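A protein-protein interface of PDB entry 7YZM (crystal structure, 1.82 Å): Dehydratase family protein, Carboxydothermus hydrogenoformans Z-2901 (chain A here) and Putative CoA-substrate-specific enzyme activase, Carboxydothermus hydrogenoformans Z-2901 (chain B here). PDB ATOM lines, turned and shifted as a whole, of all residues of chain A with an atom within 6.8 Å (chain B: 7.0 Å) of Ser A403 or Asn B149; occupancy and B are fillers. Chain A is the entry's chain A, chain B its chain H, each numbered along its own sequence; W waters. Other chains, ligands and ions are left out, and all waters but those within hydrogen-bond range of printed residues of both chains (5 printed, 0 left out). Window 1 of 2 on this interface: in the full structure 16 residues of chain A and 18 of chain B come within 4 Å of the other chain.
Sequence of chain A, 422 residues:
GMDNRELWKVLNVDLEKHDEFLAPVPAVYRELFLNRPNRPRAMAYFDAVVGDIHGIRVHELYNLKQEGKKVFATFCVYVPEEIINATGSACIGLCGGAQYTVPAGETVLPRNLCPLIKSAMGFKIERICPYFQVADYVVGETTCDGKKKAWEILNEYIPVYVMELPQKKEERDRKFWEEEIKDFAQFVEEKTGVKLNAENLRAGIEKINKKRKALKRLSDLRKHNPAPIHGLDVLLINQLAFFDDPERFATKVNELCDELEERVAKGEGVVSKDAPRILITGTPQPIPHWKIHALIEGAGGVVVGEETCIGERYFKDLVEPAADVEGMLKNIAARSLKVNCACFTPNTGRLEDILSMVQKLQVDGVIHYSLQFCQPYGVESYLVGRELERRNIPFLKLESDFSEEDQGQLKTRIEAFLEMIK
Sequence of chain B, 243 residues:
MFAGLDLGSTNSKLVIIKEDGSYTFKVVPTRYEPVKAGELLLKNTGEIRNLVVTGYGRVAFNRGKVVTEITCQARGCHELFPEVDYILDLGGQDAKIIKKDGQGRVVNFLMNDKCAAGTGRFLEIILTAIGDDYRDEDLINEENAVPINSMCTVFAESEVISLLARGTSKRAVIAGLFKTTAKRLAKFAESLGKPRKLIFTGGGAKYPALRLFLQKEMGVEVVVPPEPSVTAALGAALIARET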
ATOM      1  N   ALA A  98      12.559   1.434  29.318  1.00  0.00           N
ATOM      2  CA  ALA A  98      13.679   0.944  28.528  1.00  0.00           C
ATOM      3  C   ALA A  98      13.223   0.243  27.258  1.00  0.00           C
ATOM      4  O   ALA A  98      12.384  -0.665  27.300  1.00  0.00           O
ATOM      5  CB  ALA A  98      14.550  -0.016  29.347  1.00  0.00           C
ATOM      6  N   GLN A  99      13.820   0.642  26.132  1.00  0.00           N
ATOM      7  CA  GLN A  99      13.545  -0.036  24.871  1.00  0.00           C
ATOM      8  C   GLN A  99      14.075  -1.464  24.866  1.00  0.00           C
ATOM      9  O   GLN A  99      13.551  -2.312  24.132  1.00  0.00           O
ATOM     10  CB  GLN A  99      14.164   0.745  23.712  1.00  0.00           C
ATOM     11  CG  GLN A  99      13.919   0.122  22.340  1.00  0.00           C
ATOM     12  CD  GLN A  99      12.469   0.207  21.894  1.00  0.00           C
ATOM     13  OE1 GLN A  99      11.727   1.091  22.320  1.00  0.00           O
ATOM     14  NE2 GLN A  99      12.059  -0.718  21.031  1.00  0.00           N
ATOM     15  N   PRO A 115       4.643   1.695  25.283  1.00  0.00           N
ATOM     16  CA  PRO A 115       5.948   1.103  25.616  1.00  0.00           C
ATOM     17  C   PRO A 115       6.187   0.959  27.108  1.00  0.00           C
ATOM     18  O   PRO A 115       6.982   0.101  27.504  1.00  0.00           O
ATOM     19  CB  PRO A 115       6.951   2.072  24.976  1.00  0.00           C
ATOM     20  CG  PRO A 115       6.212   3.349  24.787  1.00  0.00           C
ATOM     21  CD  PRO A 115       4.771   2.992  24.592  1.00  0.00           C
ATOM     22  N   HIS A 289      13.998   7.359  30.769  1.00  0.00           N
ATOM     23  CA  HIS A 289      13.403   8.031  29.613  1.00  0.00           C
ATOM     24  C   HIS A 289      13.622   9.537  29.744  1.00  0.00           C
ATOM     25  O   HIS A 289      12.720  10.308  30.075  1.00  0.00           O
ATOM     26  CB  HIS A 289      11.931   7.671  29.507  1.00  0.00           C
ATOM     27  CG  HIS A 289      11.288   8.112  28.231  1.00  0.00           C
ATOM     28  ND1 HIS A 289      11.828   7.847  26.992  1.00  0.00           N
ATOM     29  CD2 HIS A 289      10.140   8.791  28.005  1.00  0.00           C
ATOM     30  CE1 HIS A 289      11.040   8.347  26.057  1.00  0.00           C
ATOM     31  NE2 HIS A 289      10.008   8.923  26.645  1.00  0.00           N
ATOM     32  N   LYS A 291      14.874  11.582  27.248  1.00  0.00           N
ATOM     33  CA  LYS A 291      15.064  12.180  25.927  1.00  0.00           C
ATOM     34  C   LYS A 291      14.455  13.577  25.815  1.00  0.00           C
ATOM     35  O   LYS A 291      15.120  14.518  25.372  1.00  0.00           O
ATOM     36  CB  LYS A 291      14.454  11.236  24.892  1.00  0.00           C
ATOM     37  CG  LYS A 291      14.443  11.696  23.458  1.00  0.00           C
ATOM     38  CD  LYS A 291      14.155  10.498  22.535  1.00  0.00           C
ATOM     39  CE  LYS A 291      12.751   9.924  22.747  1.00  0.00           C
ATOM     40  NZ  LYS A 291      12.445   8.760  21.853  1.00  0.00           N
ATOM     41  N   SER A 400       6.337   9.947  21.335  1.00  0.00           N
ATOM     42  CA  SER A 400       7.483   9.112  20.992  1.00  0.00           C
ATOM     43  C   SER A 400       7.396   7.809  21.779  1.00  0.00           C
ATOM     44  O   SER A 400       6.461   7.587  22.551  1.00  0.00           O
ATOM     45  CB  SER A 400       8.797   9.849  21.272  1.00  0.00           C
ATOM     46  OG  SER A 400       9.903   9.154  20.723  1.00  0.00           O
ATOM     47  N   ASP A 401       8.377   6.940  21.557  1.00  0.00           N
ATOM     48  CA  ASP A 401       8.507   5.713  22.332  1.00  0.00           C
ATOM     49  C   ASP A 401       9.876   5.714  23.002  1.00  0.00           C
ATOM     50  O   ASP A 401      10.533   6.758  23.088  1.00  0.00           O
ATOM     51  CB  ASP A 401       8.296   4.475  21.452  1.00  0.00           C
ATOM     52  CG  ASP A 401       9.231   4.422  20.256  1.00  0.00           C
ATOM     53  OD1 ASP A 401      10.386   4.883  20.371  1.00  0.00           O
ATOM     54  OD2 ASP A 401       8.808   3.902  19.198  1.00  0.00           O
ATOM     55  N   PHE A 402      10.330   4.558  23.475  1.00  0.00           N
ATOM     56  CA  PHE A 402      11.576   4.507  24.221  1.00  0.00           C
ATOM     57  C   PHE A 402      12.798   4.383  23.323  1.00  0.00           C
ATOM     58  O   PHE A 402      13.927   4.437  23.822  1.00  0.00           O
ATOM     59  CB  PHE A 402      11.529   3.345  25.216  1.00  0.00           C
ATOM     60  CG  PHE A 402      10.490   3.512  26.302  1.00  0.00           C
ATOM     61  CD1 PHE A 402      10.031   4.766  26.669  1.00  0.00           C
ATOM     62  CD2 PHE A 402       9.986   2.404  26.964  1.00  0.00           C
ATOM     63  CE1 PHE A 402       9.078   4.904  27.670  1.00  0.00           C
ATOM     64  CE2 PHE A 402       9.043   2.540  27.963  1.00  0.00           C
ATOM     65  CZ  PHE A 402       8.593   3.784  28.317  1.00  0.00           C
ATOM     66  N   SER A 403      12.601   4.217  22.020  1.00  0.00           N
ATOM     67  CA  SER A 403      13.731   4.146  21.108  1.00  0.00           C
ATOM     68  C   SER A 403      14.407   5.506  21.059  1.00  0.00           C
ATOM     69  O   SER A 403      13.752   6.529  20.854  1.00  0.00           O
ATOM     70  CB  SER A 403      13.275   3.717  19.718  1.00  0.00           C
ATOM     71  OG  SER A 403      14.400   3.595  18.871  1.00  0.00           O
ATOM     72  N   GLU A 404      15.722   5.520  21.260  1.00  0.00           N
ATOM     73  CA  GLU A 404      16.413   6.776  21.504  1.00  0.00           C
ATOM     74  C   GLU A 404      16.747   7.552  20.240  1.00  0.00           C
ATOM     75  O   GLU A 404      17.158   8.710  20.349  1.00  0.00           O
ATOM     76  CB  GLU A 404      17.725   6.539  22.261  1.00  0.00           C
ATOM     77  CG  GLU A 404      17.657   5.516  23.370  1.00  0.00           C
ATOM     78  CD  GLU A 404      17.712   6.152  24.742  1.00  0.00           C
ATOM     79  OE1 GLU A 404      18.239   5.507  25.676  1.00  0.00           O
ATOM     80  OE2 GLU A 404      17.227   7.296  24.886  1.00  0.00           O
ATOM     81  N   GLU A 405      16.612   6.959  19.057  1.00  0.00           N
ATOM     82  CA  GLU A 405      17.274   7.504  17.879  1.00  0.00           C
ATOM     83  C   GLU A 405      16.354   8.312  16.968  1.00  0.00           C
ATOM     84  O   GLU A 405      16.776   8.699  15.876  1.00  0.00           O
ATOM     85  CB  GLU A 405      17.942   6.379  17.087  1.00  0.00           C
ATOM     86  CG  GLU A 405      18.967   5.563  17.875  1.00  0.00           C
ATOM     87  CD  GLU A 405      20.028   6.404  18.585  1.00  0.00           C
ATOM     88  OE1 GLU A 405      20.670   5.864  19.515  1.00  0.00           O
ATOM     89  OE2 GLU A 405      20.236   7.587  18.220  1.00  0.00           O
ATOM     90  N   ASP A 406      15.145   8.650  17.413  1.00  0.00           N
ATOM     91  CA  ASP A 406      14.321   9.627  16.701  1.00  0.00           C
ATOM     92  C   ASP A 406      14.663  11.026  17.225  1.00  0.00           C
ATOM     93  O   ASP A 406      13.824  11.942  17.193  1.00  0.00           O
ATOM     94  CB  ASP A 406      12.826   9.322  16.839  1.00  0.00           C
ATOM     95  CG  ASP A 406      12.310   9.519  18.279  1.00  0.00           C
ATOM     96  OD1 ASP A 406      13.125   9.458  19.231  1.00  0.00           O
ATOM     97  OD2 ASP A 406      11.083   9.712  18.445  1.00  0.00           O
ATOM     98  N   GLN A 407      15.923  11.224  17.628  1.00  0.00           N
ATOM     99  CA  GLN A 407      16.369  12.519  18.150  1.00  0.00           C
ATOM    100  C   GLN A 407      16.182  13.649  17.143  1.00  0.00           C
ATOM    101  O   GLN A 407      15.769  14.758  17.505  1.00  0.00           O
ATOM    102  CB  GLN A 407      17.856  12.476  18.530  1.00  0.00           C
ATOM    103  CG  GLN A 407      18.263  11.374  19.474  1.00  0.00           C
ATOM    104  CD  GLN A 407      18.457  11.874  20.896  1.00  0.00           C
ATOM    105  OE1 GLN A 407      18.993  12.963  21.122  1.00  0.00           O
ATOM    106  NE2 GLN A 407      18.023  11.075  21.864  1.00  0.00           N
ATOM    107  N   LEU A 410      12.503  14.838  16.760  1.00  0.00           N
ATOM    108  CA  LEU A 410      12.063  15.567  17.945  1.00  0.00           C
ATOM    109  C   LEU A 410      12.814  16.880  18.101  1.00  0.00           C
ATOM    110  O   LEU A 410      12.235  17.882  18.532  1.00  0.00           O
ATOM    111  CB  LEU A 410      12.250  14.703  19.188  1.00  0.00           C
ATOM    112  CG  LEU A 410      11.320  13.502  19.318  1.00  0.00           C
ATOM    113  CD1 LEU A 410      11.868  12.570  20.396  1.00  0.00           C
ATOM    114  CD2 LEU A 410       9.902  13.940  19.626  1.00  0.00           C
ATOM    115  N   VAL B 146      24.134   0.104  16.575  1.00  0.00           N
ATOM    116  CA  VAL B 146      23.177   1.050  17.140  1.00  0.00           C
ATOM    117  C   VAL B 146      21.815   0.365  17.194  1.00  0.00           C
ATOM    118  O   VAL B 146      21.321  -0.080  16.148  1.00  0.00           O
ATOM    119  CB  VAL B 146      23.110   2.337  16.311  1.00  0.00           C
ATOM    120  CG1 VAL B 146      22.068   3.285  16.887  1.00  0.00           C
ATOM    121  CG2 VAL B 146      24.478   2.994  16.264  1.00  0.00           C
ATOM    122  N   PRO B 147      21.186   0.252  18.367  1.00  0.00           N
ATOM    123  CA  PRO B 147      19.805  -0.247  18.401  1.00  0.00           C
ATOM    124  C   PRO B 147      18.888   0.688  17.624  1.00  0.00           C
ATOM    125  O   PRO B 147      18.900   1.906  17.822  1.00  0.00           O
ATOM    126  CB  PRO B 147      19.463  -0.277  19.897  1.00  0.00           C
ATOM    127  CG  PRO B 147      20.781  -0.256  20.605  1.00  0.00           C
ATOM    128  CD  PRO B 147      21.718   0.512  19.717  1.00  0.00           C
ATOM    129  N   ILE B 148      18.110   0.108  16.719  1.00  0.00           N
ATOM    130  CA  ILE B 148      17.172   0.836  15.876  1.00  0.00           C
ATOM    131  C   ILE B 148      15.769   0.369  16.229  1.00  0.00           C
ATOM    132  O   ILE B 148      15.563  -0.779  16.631  1.00  0.00           O
ATOM    133  CB  ILE B 148      17.506   0.629  14.381  1.00  0.00           C
ATOM    134  CG1 ILE B 148      18.905   1.213  14.127  1.00  0.00           C
ATOM    135  CG2 ILE B 148      16.471   1.290  13.494  1.00  0.00           C
ATOM    136  CD1 ILE B 148      19.357   1.203  12.708  1.00  0.00           C
ATOM    137  N   ASN B 149      14.809   1.281  16.122  1.00  0.00           N
ATOM    138  CA  ASN B 149      13.446   0.980  16.533  1.00  0.00           C
ATOM    139  C   ASN B 149      12.948  -0.285  15.846  1.00  0.00           C
ATOM    140  O   ASN B 149      13.117  -0.454  14.639  1.00  0.00           O
ATOM    141  CB  ASN B 149      12.536   2.160  16.199  1.00  0.00           C
ATOM    142  CG  ASN B 149      11.269   2.164  17.021  1.00  0.00           C
ATOM    143  OD1 ASN B 149      10.731   1.108  17.360  1.00  0.00           O
ATOM    144  ND2 ASN B 149      10.791   3.353  17.360  1.00  0.00           N
ATOM    145  N   SER B 150      12.333  -1.175  16.625  1.00  0.00           N
ATOM    146  CA  SER B 150      11.825  -2.441  16.110  1.00  0.00           C
ATOM    147  C   SER B 150      10.351  -2.376  15.718  1.00  0.00           C
ATOM    148  O   SER B 150       9.766  -3.405  15.366  1.00  0.00           O
ATOM    149  CB  SER B 150      12.024  -3.551  17.149  1.00  0.00           C
ATOM    150  OG  SER B 150      11.534  -3.159  18.422  1.00  0.00           O
ATOM    151  N   MET B 151       9.736  -1.198  15.764  1.00  0.00           N
ATOM    152  CA  MET B 151       8.301  -1.120  15.519  1.00  0.00           C
ATOM    153  C   MET B 151       7.957  -1.453  14.073  1.00  0.00           C
ATOM    154  O   MET B 151       7.131  -2.329  13.800  1.00  0.00           O
ATOM    155  CB  MET B 151       7.786   0.271  15.865  1.00  0.00           C
ATOM    156  CG  MET B 151       6.294   0.408  15.703  1.00  0.00           C
ATOM    157  SD  MET B 151       5.586  -0.081  17.296  1.00  0.00           S
ATOM    158  CE  MET B 151       4.239  -1.094  16.797  1.00  0.00           C
ATOM    159  N   CYS B 152       8.559  -0.737  13.132  1.00  0.00           N
ATOM    160  CA  CYS B 152       8.159  -0.818  11.735  1.00  0.00           C
ATOM    161  C   CYS B 152       9.222  -0.112  10.906  1.00  0.00           C
ATOM    162  O   CYS B 152      10.124   0.540  11.437  1.00  0.00           O
ATOM    163  CB  CYS B 152       6.790  -0.175  11.516  1.00  0.00           C
ATOM    164  SG  CYS B 152       6.863   1.602  11.870  1.00  0.00           S
ATOM    165  N   THR B 153       9.086  -0.236   9.589  1.00  0.00           N
ATOM    166  CA  THR B 153      10.055   0.354   8.678  1.00  0.00           C
ATOM    167  C   THR B 153       9.937   1.872   8.607  1.00  0.00           C
ATOM    168  O   THR B 153      10.912   2.538   8.256  1.00  0.00           O
ATOM    169  CB  THR B 153       9.884  -0.250   7.285  1.00  0.00           C
ATOM    170  OG1 THR B 153       8.567   0.024   6.803  1.00  0.00           O
ATOM    171  CG2 THR B 153      10.113  -1.754   7.337  1.00  0.00           C
ATOM    172  N   PHE B 155       9.315   3.954  11.330  1.00  0.00           N
ATOM    173  CA  PHE B 155      10.078   4.473  12.460  1.00  0.00           C
ATOM    174  C   PHE B 155      11.563   4.200  12.273  1.00  0.00           C
ATOM    175  O   PHE B 155      12.406   5.019  12.653  1.00  0.00           O
ATOM    176  CB  PHE B 155       9.610   3.843  13.776  1.00  0.00           C
ATOM    177  CG  PHE B 155       8.215   4.215  14.193  1.00  0.00           C
ATOM    178  CD1 PHE B 155       7.341   4.839  13.321  1.00  0.00           C
ATOM    179  CD2 PHE B 155       7.774   3.913  15.470  1.00  0.00           C
ATOM    180  CE1 PHE B 155       6.054   5.149  13.712  1.00  0.00           C
ATOM    181  CE2 PHE B 155       6.493   4.235  15.872  1.00  0.00           C
ATOM    182  CZ  PHE B 155       5.629   4.851  14.989  1.00  0.00           C
ATOM    183  N   ALA B 156      11.903   3.045  11.692  1.00  0.00           N
ATOM    184  CA  ALA B 156      13.308   2.699  11.505  1.00  0.00           C
ATOM    185  C   ALA B 156      13.971   3.595  10.464  1.00  0.00           C
ATOM    186  O   ALA B 156      15.126   4.001  10.635  1.00  0.00           O
ATOM    187  CB  ALA B 156      13.441   1.231  11.104  1.00  0.00           C
ATOM    188  N   GLU B 157      13.266   3.903   9.371  1.00  0.00           N
ATOM    189  CA  GLU B 157      13.810   4.857   8.412  1.00  0.00           C
ATOM    190  C   GLU B 157      14.046   6.211   9.075  1.00  0.00           C
ATOM    191  O   GLU B 157      15.092   6.836   8.873  1.00  0.00           O
ATOM    192  CB  GLU B 157      12.876   5.004   7.209  1.00  0.00           C
ATOM    193  CG  GLU B 157      13.376   6.023   6.170  1.00  0.00           C
ATOM    194  CD  GLU B 157      12.358   6.343   5.074  1.00  0.00           C
ATOM    195  OE1 GLU B 157      11.175   5.962   5.209  1.00  0.00           O
ATOM    196  OE2 GLU B 157      12.746   6.988   4.073  1.00  0.00           O
ATOM    197  N   GLU B 159      14.828   6.829  12.046  1.00  0.00           N
ATOM    198  CA  GLU B 159      16.015   6.767  12.895  1.00  0.00           C
ATOM    199  C   GLU B 159      17.288   6.669  12.069  1.00  0.00           C
ATOM    200  O   GLU B 159      18.322   7.242  12.436  1.00  0.00           O
ATOM    201  CB  GLU B 159      15.907   5.582  13.863  1.00  0.00           C
ATOM    202  CG  GLU B 159      14.764   5.740  14.844  1.00  0.00           C
ATOM    203  CD  GLU B 159      14.870   4.836  16.057  1.00  0.00           C
ATOM    204  OE1 GLU B 159      15.638   3.851  16.017  1.00  0.00           O
ATOM    205  OE2 GLU B 159      14.164   5.116  17.051  1.00  0.00           O
ATOM    206  N   LEU B 177      20.832  -2.381  12.178  1.00  0.00           N
ATOM    207  CA  LEU B 177      19.647  -2.817  11.445  1.00  0.00           C
ATOM    208  C   LEU B 177      19.535  -4.340  11.423  1.00  0.00           C
ATOM    209  O   LEU B 177      18.459  -4.893  11.671  1.00  0.00           O
ATOM    210  CB  LEU B 177      19.676  -2.265  10.020  1.00  0.00           C
ATOM    211  CG  LEU B 177      19.226  -0.822   9.804  1.00  0.00           C
ATOM    212  CD1 LEU B 177      19.678  -0.365   8.425  1.00  0.00           C
ATOM    213  CD2 LEU B 177      17.723  -0.676   9.955  1.00  0.00           C
ATOM    214  N   THR B 180      18.829  -5.625  15.199  1.00  0.00           N
ATOM    215  CA  THR B 180      17.458  -5.446  15.666  1.00  0.00           C
ATOM    216  C   THR B 180      16.501  -6.342  14.894  1.00  0.00           C
ATOM    217  O   THR B 180      15.563  -6.902  15.471  1.00  0.00           O
ATOM    218  CB  THR B 180      17.053  -3.976  15.542  1.00  0.00           C
ATOM    219  OG1 THR B 180      18.003  -3.161  16.237  1.00  0.00           O
ATOM    220  CG2 THR B 180      15.669  -3.738  16.137  1.00  0.00           C
ATOM    221  N   ARG B 184      14.030  -9.138  16.615  1.00  0.00           N
ATOM    222  CA  ARG B 184      12.593  -9.270  16.387  1.00  0.00           C
ATOM    223  C   ARG B 184      12.252 -10.639  15.808  1.00  0.00           C
ATOM    224  O   ARG B 184      11.239 -11.250  16.169  1.00  0.00           O
ATOM    225  CB  ARG B 184      12.081  -8.199  15.428  1.00  0.00           C
ATOM    226  CG  ARG B 184      12.239  -6.766  15.847  1.00  0.00           C
ATOM    227  CD  ARG B 184      11.915  -5.882  14.630  1.00  0.00           C
ATOM    228  NE  ARG B 184      10.505  -5.959  14.223  1.00  0.00           N
ATOM    229  CZ  ARG B 184      10.004  -5.373  13.136  1.00  0.00           C
ATOM    230  NH1 ARG B 184       8.711  -5.478  12.849  1.00  0.00           N
ATOM    231  NH2 ARG B 184      10.796  -4.680  12.328  1.00  0.00           N
HETATM  232  O   HOH W   1      13.713  -2.942  19.997  1.00  0.00           O
HETATM  233  O   HOH W   2      16.100   1.291  19.622  1.00  0.00           O
HETATM  234  O   HOH W   3       6.169   2.542  19.245  1.00  0.00           O
HETATM  235  O   HOH W   4      19.830   3.358  20.230  1.00  0.00           O
HETATM  236  O   HOH W   5       9.527  -0.154  19.548  1.00  0.00           O
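The side-chain carboxylate (OD2) of Asp A401 is in hydrogen-bond range of the side-chain amide nitrogen (ND2) of Asn B149 (2.8 Å). The side-chain hydroxyl of Ser A403 sits close to the side-chain carboxylate of Glu B159 (3.1 Å).
OE1 of Gln A99 lies within hydrogen-bond range of N of Ser A403 (3.3 Å). NZ of Lys A291 lies within hydrogen-bond range of O of Asp A401, at 3.0 Å. OG of Ser A400 is in hydrogen-bond range of OD2 of Asp A406, 2.6 Å away. The side-chain carboxylate (OD1) of Asp A401 is in hydrogen-bond range of the backbone NH (N) of Ser A403, 2.8 Å away. N of Met B151 is in hydrogen-bond range of OD1 of Asn B149, at 3.0 Å. The backbone NH (N) of Asn B149 is in hydrogen-bond range of the side-chain carboxylate (OE1) of Glu B159 (2.7 Å).
Among the printed residues, pairs that only touch across the chains: Ser A403 with Asn B149, Glu A405 with Glu B159, Gln A99 with Ser B150, Glu A405 with Pro B147, Asp A406 with Glu B159, Asp A401 with Phe B155 and Glu A405 with Val B146.
Of the printed residues of chain B, Gln A99 touches Ser B150. Printed residues of chain B within 4 Å of Asp A401: Asn B149 and Phe B155. Of chain B, only Asn B149 (3.4 Å) and Glu B159 (2.4 Å) come within 4 Å of Ser A403. Gln A407 touches none of the printed residues of chain B. Of the printed residues of chain A, Pro B147 touches Glu A405 (3.7 Å). Of chain A, only Asp A401 and Ser A403 come within 4 Å of Asn B149. Of the printed residues of chain A, Ser B150 touches Gln A99 (3.6 Å). Printed residues of chain A within 4 Å of Phe B155: Asp A401. Glu B157 touches none of the printed residues of chain A. The nearest residue of chain B that does not touch Ser A403 is Ile B148 (4.4 Å). The nearest printed residue of chain A that does not touch Ser B150 is Ser A403 (5.7 Å).
Hydrophobic or aromatic side chains of chain B that line the printed part of chain A: Val B146 and Phe B155. Printed residues of chain A that touch a printed residue of chain B: Gln A99, Asp A401, Ser A403, Glu A405 and Asp A406. Among the printed residues, no Asp or Glu carboxylate lies within 4 Å of a Lys or Arg side-chain nitrogen of the other chain.
Water W1 lies within hydrogen-bond range of the side-chain hydroxyl of Ser B150 (2.7 Å) and the side-chain amide nitrogen of Gln A99 (3.0 Å). Water W4 lies within hydrogen-bond range of the side-chain carboxylate (OE1) of Glu A405 (2.7 Å) and the backbone carbonyl oxygen (O) of Pro B147 (3.0 Å). Water W5 lies within hydrogen-bond range of OD1 of Asn B149 and NE2 of Gln A99. Water W2 bridges the side-chain hydroxyl of Ser A403 (3.0 Å) and the backbone carbonyl oxygen of Pro B147 (3.4 Å). Water W3 bridges OD2 of Asp A401 and SD of Met B151.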
